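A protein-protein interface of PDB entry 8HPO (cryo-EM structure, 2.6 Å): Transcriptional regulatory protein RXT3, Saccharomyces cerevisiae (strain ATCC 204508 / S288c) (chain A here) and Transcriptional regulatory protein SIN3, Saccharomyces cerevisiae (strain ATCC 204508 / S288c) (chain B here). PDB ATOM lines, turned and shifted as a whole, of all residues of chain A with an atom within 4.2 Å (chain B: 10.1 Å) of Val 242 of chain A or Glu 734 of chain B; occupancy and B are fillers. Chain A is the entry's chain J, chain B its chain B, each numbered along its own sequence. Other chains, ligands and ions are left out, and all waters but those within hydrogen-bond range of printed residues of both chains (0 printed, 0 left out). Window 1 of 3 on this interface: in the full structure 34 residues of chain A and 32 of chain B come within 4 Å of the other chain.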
ATOM      1  N   ASN A  66     -27.790  -4.631   3.597  1.00  0.00           N
ATOM      2  CA  ASN A  66     -26.997  -3.939   4.612  1.00  0.00           C
ATOM      3  C   ASN A  66     -25.951  -4.905   5.156  1.00  0.00           C
ATOM      4  O   ASN A  66     -26.189  -5.691   6.076  1.00  0.00           O
ATOM      5  CB  ASN A  66     -27.889  -3.384   5.715  1.00  0.00           C
ATOM      6  CG  ASN A  66     -29.074  -4.280   6.016  1.00  0.00           C
ATOM      7  OD1 ASN A  66     -29.953  -4.468   5.176  1.00  0.00           O
ATOM      8  ND2 ASN A  66     -29.105  -4.838   7.221  1.00  0.00           N
ATOM      9  N   VAL A  67     -24.767  -4.837   4.562  1.00  0.00           N
ATOM     10  CA  VAL A  67     -23.635  -5.634   5.017  1.00  0.00           C
ATOM     11  C   VAL A  67     -23.007  -4.965   6.231  1.00  0.00           C
ATOM     12  O   VAL A  67     -22.964  -3.735   6.341  1.00  0.00           O
ATOM     13  CB  VAL A  67     -22.618  -5.824   3.873  1.00  0.00           C
ATOM     14  CG1 VAL A  67     -23.294  -6.452   2.670  1.00  0.00           C
ATOM     15  CG2 VAL A  67     -22.011  -4.497   3.484  1.00  0.00           C
ATOM     16  N   SER A  68     -22.518  -5.782   7.158  1.00  0.00           N
ATOM     17  CA  SER A  68     -22.006  -5.304   8.435  1.00  0.00           C
ATOM     18  C   SER A  68     -20.594  -5.822   8.658  1.00  0.00           C
ATOM     19  O   SER A  68     -20.325  -7.008   8.451  1.00  0.00           O
ATOM     20  CB  SER A  68     -22.911  -5.744   9.587  1.00  0.00           C
ATOM     21  OG  SER A  68     -22.151  -5.999  10.754  1.00  0.00           O
ATOM     22  N   CYS A 168     -18.040  -8.920  -0.115  1.00  0.00           N
ATOM     23  CA  CYS A 168     -18.622  -7.584  -0.061  1.00  0.00           C
ATOM     24  C   CYS A 168     -18.183  -6.857   1.199  1.00  0.00           C
ATOM     25  O   CYS A 168     -18.393  -7.350   2.310  1.00  0.00           O
ATOM     26  CB  CYS A 168     -20.147  -7.624  -0.120  1.00  0.00           C
ATOM     27  SG  CYS A 168     -20.817  -6.140  -0.881  1.00  0.00           S
ATOM     28  N   HIS A 183     -16.710  -1.317  -6.452  1.00  0.00           N
ATOM     29  CA  HIS A 183     -17.709  -1.990  -5.630  1.00  0.00           C
ATOM     30  C   HIS A 183     -18.061  -1.198  -4.381  1.00  0.00           C
ATOM     31  O   HIS A 183     -19.001  -1.572  -3.673  1.00  0.00           O
ATOM     32  CB  HIS A 183     -17.211  -3.384  -5.241  1.00  0.00           C
ATOM     33  CG  HIS A 183     -18.275  -4.440  -5.253  1.00  0.00           C
ATOM     34  ND1 HIS A 183     -18.741  -5.038  -4.103  1.00  0.00           N
ATOM     35  CD2 HIS A 183     -18.948  -5.018  -6.273  1.00  0.00           C
ATOM     36  CE1 HIS A 183     -19.661  -5.930  -4.415  1.00  0.00           C
ATOM     37  NE2 HIS A 183     -19.806  -5.938  -5.725  1.00  0.00           N
ATOM     38  N   PRO A 240     -19.748 -13.477   0.381  1.00  0.00           N
ATOM     39  CA  PRO A 240     -20.988 -13.539  -0.392  1.00  0.00           C
ATOM     40  C   PRO A 240     -20.895 -12.774  -1.702  1.00  0.00           C
ATOM     41  O   PRO A 240     -20.102 -11.847  -1.866  1.00  0.00           O
ATOM     42  CB  PRO A 240     -22.003 -12.887   0.545  1.00  0.00           C
ATOM     43  CG  PRO A 240     -21.197 -11.867   1.261  1.00  0.00           C
ATOM     44  CD  PRO A 240     -19.816 -12.449   1.434  1.00  0.00           C
ATOM     45  N   SER A 241     -21.732 -13.193  -2.645  1.00  0.00           N
ATOM     46  CA  SER A 241     -21.916 -12.476  -3.898  1.00  0.00           C
ATOM     47  C   SER A 241     -22.951 -11.375  -3.691  1.00  0.00           C
ATOM     48  O   SER A 241     -24.116 -11.663  -3.398  1.00  0.00           O
ATOM     49  CB  SER A 241     -22.364 -13.432  -4.999  1.00  0.00           C
ATOM     50  OG  SER A 241     -22.174 -12.865  -6.280  1.00  0.00           O
ATOM     51  N   VAL A 242     -22.530 -10.121  -3.842  1.00  0.00           N
ATOM     52  CA  VAL A 242     -23.405  -8.970  -3.650  1.00  0.00           C
ATOM     53  C   VAL A 242     -23.224  -8.031  -4.830  1.00  0.00           C
ATOM     54  O   VAL A 242     -22.108  -7.565  -5.090  1.00  0.00           O
ATOM     55  CB  VAL A 242     -23.112  -8.227  -2.337  1.00  0.00           C
ATOM     56  CG1 VAL A 242     -23.971  -6.990  -2.242  1.00  0.00           C
ATOM     57  CG2 VAL A 242     -23.343  -9.129  -1.142  1.00  0.00           C
ATOM     58  N   LYS A 243     -24.315  -7.738  -5.531  1.00  0.00           N
ATOM     59  CA  LYS A 243     -24.259  -6.870  -6.698  1.00  0.00           C
ATOM     60  C   LYS A 243     -24.377  -5.412  -6.273  1.00  0.00           C
ATOM     61  O   LYS A 243     -25.363  -5.020  -5.644  1.00  0.00           O
ATOM     62  CB  LYS A 243     -25.364  -7.226  -7.684  1.00  0.00           C
ATOM     63  CG  LYS A 243     -25.534  -6.200  -8.782  1.00  0.00           C
ATOM     64  CD  LYS A 243     -26.328  -6.767  -9.942  1.00  0.00           C
ATOM     65  CE  LYS A 243     -25.890  -6.147 -11.257  1.00  0.00           C
ATOM     66  NZ  LYS A 243     -26.583  -6.770 -12.415  1.00  0.00           N
ATOM     67  N   ARG A 244     -23.368  -4.615  -6.612  1.00  0.00           N
ATOM     68  CA  ARG A 244     -23.410  -3.173  -6.442  1.00  0.00           C
ATOM     69  C   ARG A 244     -22.872  -2.519  -7.702  1.00  0.00           C
ATOM     70  O   ARG A 244     -21.871  -2.967  -8.263  1.00  0.00           O
ATOM     71  CB  ARG A 244     -22.559  -2.681  -5.266  1.00  0.00           C
ATOM     72  CG  ARG A 244     -22.917  -3.166  -3.879  1.00  0.00           C
ATOM     73  CD  ARG A 244     -21.778  -2.753  -2.974  1.00  0.00           C
ATOM     74  NE  ARG A 244     -22.049  -2.861  -1.551  1.00  0.00           N
ATOM     75  CZ  ARG A 244     -21.216  -2.417  -0.618  1.00  0.00           C
ATOM     76  NH1 ARG A 244     -20.074  -1.843  -0.972  1.00  0.00           N
ATOM     77  NH2 ARG A 244     -21.516  -2.543   0.666  1.00  0.00           N
ATOM     78  N   ILE A 247     -21.563  -4.536 -10.595  1.00  0.00           N
ATOM     79  CA  ILE A 247     -20.470  -5.479 -10.382  1.00  0.00           C
ATOM     80  C   ILE A 247     -20.977  -6.578  -9.462  1.00  0.00           C
ATOM     81  O   ILE A 247     -20.993  -6.405  -8.238  1.00  0.00           O
ATOM     82  CB  ILE A 247     -19.225  -4.817  -9.783  1.00  0.00           C
ATOM     83  CG1 ILE A 247     -18.663  -3.773 -10.740  1.00  0.00           C
ATOM     84  CG2 ILE A 247     -18.179  -5.866  -9.495  1.00  0.00           C
ATOM     85  CD1 ILE A 247     -17.212  -3.464 -10.510  1.00  0.00           C
ATOM     86  N   SER A 249     -20.193  -9.582  -7.622  1.00  0.00           N
ATOM     87  CA  SER A 249     -18.957 -10.211  -7.189  1.00  0.00           C
ATOM     88  C   SER A 249     -19.103 -11.731  -7.165  1.00  0.00           C
ATOM     89  O   SER A 249     -20.201 -12.284  -7.253  1.00  0.00           O
ATOM     90  CB  SER A 249     -18.539  -9.685  -5.819  1.00  0.00           C
ATOM     91  OG  SER A 249     -19.624  -9.694  -4.912  1.00  0.00           O
ATOM     92  N   ASP B 700     -31.055 -14.359 -12.233  1.00  0.00           N
ATOM     93  CA  ASP B 700     -31.619 -13.305 -11.396  1.00  0.00           C
ATOM     94  C   ASP B 700     -31.988 -12.082 -12.225  1.00  0.00           C
ATOM     95  O   ASP B 700     -33.032 -11.458 -11.999  1.00  0.00           O
ATOM     96  CB  ASP B 700     -30.627 -12.929 -10.301  1.00  0.00           C
ATOM     97  CG  ASP B 700     -29.225 -12.752 -10.835  1.00  0.00           C
ATOM     98  OD1 ASP B 700     -28.923 -13.330 -11.901  1.00  0.00           O
ATOM     99  OD2 ASP B 700     -28.429 -12.034 -10.199  1.00  0.00           O
ATOM    100  N   LYS B 729     -33.598 -14.473  -2.427  1.00  0.00           N
ATOM    101  CA  LYS B 729     -32.355 -14.041  -1.792  1.00  0.00           C
ATOM    102  C   LYS B 729     -32.702 -13.236  -0.540  1.00  0.00           C
ATOM    103  O   LYS B 729     -32.317 -12.081  -0.358  1.00  0.00           O
ATOM    104  CB  LYS B 729     -31.493 -13.253  -2.774  1.00  0.00           C
ATOM    105  CG  LYS B 729     -32.208 -12.142  -3.540  1.00  0.00           C
ATOM    106  CD  LYS B 729     -31.820 -10.760  -3.024  1.00  0.00           C
ATOM    107  CE  LYS B 729     -32.711  -9.674  -3.601  1.00  0.00           C
ATOM    108  NZ  LYS B 729     -32.749  -8.470  -2.727  1.00  0.00           N
ATOM    109  N   THR B 730     -33.425 -13.901   0.363  1.00  0.00           N
ATOM    110  CA  THR B 730     -34.008 -13.238   1.528  1.00  0.00           C
ATOM    111  C   THR B 730     -32.899 -12.882   2.517  1.00  0.00           C
ATOM    112  O   THR B 730     -32.787 -13.419   3.618  1.00  0.00           O
ATOM    113  CB  THR B 730     -35.070 -14.118   2.173  1.00  0.00           C
ATOM    114  OG1 THR B 730     -35.974 -14.592   1.168  1.00  0.00           O
ATOM    115  CG2 THR B 730     -35.860 -13.326   3.211  1.00  0.00           C
ATOM    116  N   LYS B 731     -32.059 -11.953   2.082  1.00  0.00           N
ATOM    117  CA  LYS B 731     -30.905 -11.522   2.847  1.00  0.00           C
ATOM    118  C   LYS B 731     -30.636 -10.054   2.564  1.00  0.00           C
ATOM    119  O   LYS B 731     -30.218  -9.693   1.460  1.00  0.00           O
ATOM    120  CB  LYS B 731     -29.680 -12.369   2.509  1.00  0.00           C
ATOM    121  CG  LYS B 731     -28.560 -12.269   3.525  1.00  0.00           C
ATOM    122  CD  LYS B 731     -29.094 -12.017   4.924  1.00  0.00           C
ATOM    123  CE  LYS B 731     -29.603 -13.290   5.586  1.00  0.00           C
ATOM    124  NZ  LYS B 731     -29.755 -13.112   7.059  1.00  0.00           N
ATOM    125  N   CYS B 732     -30.893  -9.217   3.560  1.00  0.00           N
ATOM    126  CA  CYS B 732     -30.371  -7.862   3.582  1.00  0.00           C
ATOM    127  C   CYS B 732     -29.575  -7.713   4.867  1.00  0.00           C
ATOM    128  O   CYS B 732     -28.584  -6.980   4.919  1.00  0.00           O
ATOM    129  CB  CYS B 732     -31.504  -6.838   3.497  1.00  0.00           C
ATOM    130  SG  CYS B 732     -32.945  -7.420   2.577  1.00  0.00           S
ATOM    131  N   ILE B 733     -29.997  -8.437   5.902  1.00  0.00           N
ATOM    132  CA  ILE B 733     -29.299  -8.470   7.181  1.00  0.00           C
ATOM    133  C   ILE B 733     -28.286  -9.604   7.169  1.00  0.00           C
ATOM    134  O   ILE B 733     -28.559 -10.696   7.679  1.00  0.00           O
ATOM    135  CB  ILE B 733     -30.282  -8.651   8.352  1.00  0.00           C
ATOM    136  CG1 ILE B 733     -31.556  -7.841   8.114  1.00  0.00           C
ATOM    137  CG2 ILE B 733     -29.616  -8.264   9.661  1.00  0.00           C
ATOM    138  CD1 ILE B 733     -32.743  -8.684   7.694  1.00  0.00           C
ATOM    139  N   GLU B 734     -27.105  -9.353   6.614  1.00  0.00           N
ATOM    140  CA  GLU B 734     -26.037 -10.342   6.583  1.00  0.00           C
ATOM    141  C   GLU B 734     -24.780  -9.729   7.174  1.00  0.00           C
ATOM    142  O   GLU B 734     -24.287  -8.710   6.677  1.00  0.00           O
ATOM    143  CB  GLU B 734     -25.767 -10.837   5.161  1.00  0.00           C
ATOM    144  CG  GLU B 734     -25.846  -9.762   4.102  1.00  0.00           C
ATOM    145  CD  GLU B 734     -24.523  -9.544   3.411  1.00  0.00           C
ATOM    146  OE1 GLU B 734     -24.492  -9.564   2.164  1.00  0.00           O
ATOM    147  OE2 GLU B 734     -23.511  -9.363   4.114  1.00  0.00           O
ATOM    148  N   ASN B 735     -24.269 -10.344   8.231  1.00  0.00           N
ATOM    149  CA  ASN B 735     -23.014  -9.940   8.840  1.00  0.00           C
ATOM    150  C   ASN B 735     -21.925 -10.875   8.343  1.00  0.00           C
ATOM    151  O   ASN B 735     -22.003 -12.089   8.556  1.00  0.00           O
ATOM    152  CB  ASN B 735     -23.095  -9.978  10.368  1.00  0.00           C
ATOM    153  CG  ASN B 735     -21.876  -9.362  11.037  1.00  0.00           C
ATOM    154  OD1 ASN B 735     -21.624  -9.588  12.221  1.00  0.00           O
ATOM    155  ND2 ASN B 735     -21.119  -8.575  10.280  1.00  0.00           N
ATOM    156  N   ILE B 736     -20.921 -10.314   7.670  1.00  0.00           N
ATOM    157  CA  ILE B 736     -19.776 -11.128   7.297  1.00  0.00           C
ATOM    158  C   ILE B 736     -19.032 -11.500   8.569  1.00  0.00           C
ATOM    159  O   ILE B 736     -18.395 -10.661   9.218  1.00  0.00           O
ATOM    160  CB  ILE B 736     -18.882 -10.392   6.285  1.00  0.00           C
ATOM    161  CG1 ILE B 736     -18.527  -8.992   6.777  1.00  0.00           C
ATOM    162  CG2 ILE B 736     -19.569 -10.311   4.933  1.00  0.00           C
ATOM    163  CD1 ILE B 736     -17.606  -8.252   5.865  1.00  0.00           C
ATOM    164  N   VAL B 737     -19.148 -12.764   8.957  1.00  0.00           N
ATOM    165  CA  VAL B 737     -18.699 -13.228  10.260  1.00  0.00           C
ATOM    166  C   VAL B 737     -17.234 -13.615  10.143  1.00  0.00           C
ATOM    167  O   VAL B 737     -16.718 -13.799   9.036  1.00  0.00           O
ATOM    168  CB  VAL B 737     -19.564 -14.396  10.768  1.00  0.00           C
ATOM    169  CG1 VAL B 737     -19.194 -15.693  10.076  1.00  0.00           C
ATOM    170  CG2 VAL B 737     -19.465 -14.522  12.282  1.00  0.00           C
ATOM    171  N   HIS B 738     -16.563 -13.713  11.284  1.00  0.00           N
ATOM    172  CA  HIS B 738     -15.134 -13.972  11.302  1.00  0.00           C
ATOM    173  C   HIS B 738     -14.859 -15.462  11.148  1.00  0.00           C
ATOM    174  O   HIS B 738     -15.758 -16.295  11.289  1.00  0.00           O
ATOM    175  CB  HIS B 738     -14.554 -13.439  12.610  1.00  0.00           C
ATOM    176  CG  HIS B 738     -13.062 -13.481  12.686  1.00  0.00           C
ATOM    177  ND1 HIS B 738     -12.369 -14.606  13.075  1.00  0.00           N
ATOM    178  CD2 HIS B 738     -12.133 -12.530  12.443  1.00  0.00           C
ATOM    179  CE1 HIS B 738     -11.075 -14.348  13.060  1.00  0.00           C
ATOM    180  NE2 HIS B 738     -10.906 -13.094  12.681  1.00  0.00           N
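SG of Cys 168 of chain A sits at hydrogen-bond distance from NE of Arg 244 of chain A (3.6 Å).
A ring nitrogen (NE2) of His 183 of chain A lies within hydrogen-bond range of the backbone carbonyl oxygen (O) of Val 242 of chain A, at 2.9 Å.
OG of Ser 249 of chain A lies within hydrogen-bond range of N of Val 242 of chain A.
The side-chain amino group of Lys 731 of chain B sits at hydrogen-bond distance from the backbone carbonyl oxygen of Ile 733 of chain B, at 2.8 Å.
ND2 of Asn 66 of chain A touches CA of Ile 733 of chain B, at 3.6 Å.
O of Asn 66 of chain A touches O of Glu 734 of chain B, at 3.6 Å.
Val 67 of chain A touches Glu 734 of chain B.
Ile 736 of chain B touches Cys 168 of chain A.
CG2 of Val 242 of chain A touches OE1 of Glu 734 of chain B, 3.5 Å away.
Of the printed residues of chain B, Val 242 of chain A touches Glu 734 (3.5 Å).
Glu 734 of chain B touches just these residues of chain A: Asn 66, Val 67, Ser 68 and Val 242.
Val 67 of chain A touches just one residue of chain B: Glu 734 (3.3 Å).
Of chain B, only Glu 734, Asn 735 and Ile 736 come within 4 Å of Ser 68 of chain A.
Pro 240 of chain A touches none of the printed residues of chain B.
No residue of chain B comes within 4 Å of Ser 241 of chain A.
No residue of chain B comes within 4 Å of Ser 249 of chain A.
Printed residues of chain B within 4 Å of Asn 66 of chain A: Cys 732 (2.8 Å), Ile 733 (3.6 Å) and Glu 734 (3.6 Å).
Of the printed residues of chain B, Cys 168 of chain A touches Ile 736 (3.8 Å).
Lys 243 of chain A touches none of the printed residues of chain B.
Thr 730 of chain B touches none of the printed residues of chain A.
The nearest residue of chain B that does not touch Val 242 of chain A is Ile 736 of chain B (7.2 Å).
The nearest residue of chain A that does not touch Glu 734 of chain B is Pro 240 of chain A (4.1 Å).
The backbone carbonyl oxygen of Cys 732 of chain B is in hydrogen-bond range of the backbone NH of Asn 66 of chain A (2.8 Å).
N of Ser 68 of chain A lies within hydrogen-bond range of O of Glu 734 of chain B.
ND2 of Asn 735 of chain B is in hydrogen-bond range of O of Ser 68 of chain A.
O of Ser 68 of chain A sits close to N of Ile 736 of chain B (3.4 Å).
Of the 11 printed residues of chain B, 5 touch a printed residue of chain A.
Hydrophobic or aromatic side chains of chain A that line the printed part of chain B: Val 67 and Val 242.
Among the printed residues, no Asp or Glu carboxylate lies within 4 Å of a Lys or Arg side-chain nitrogen of the other chain.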
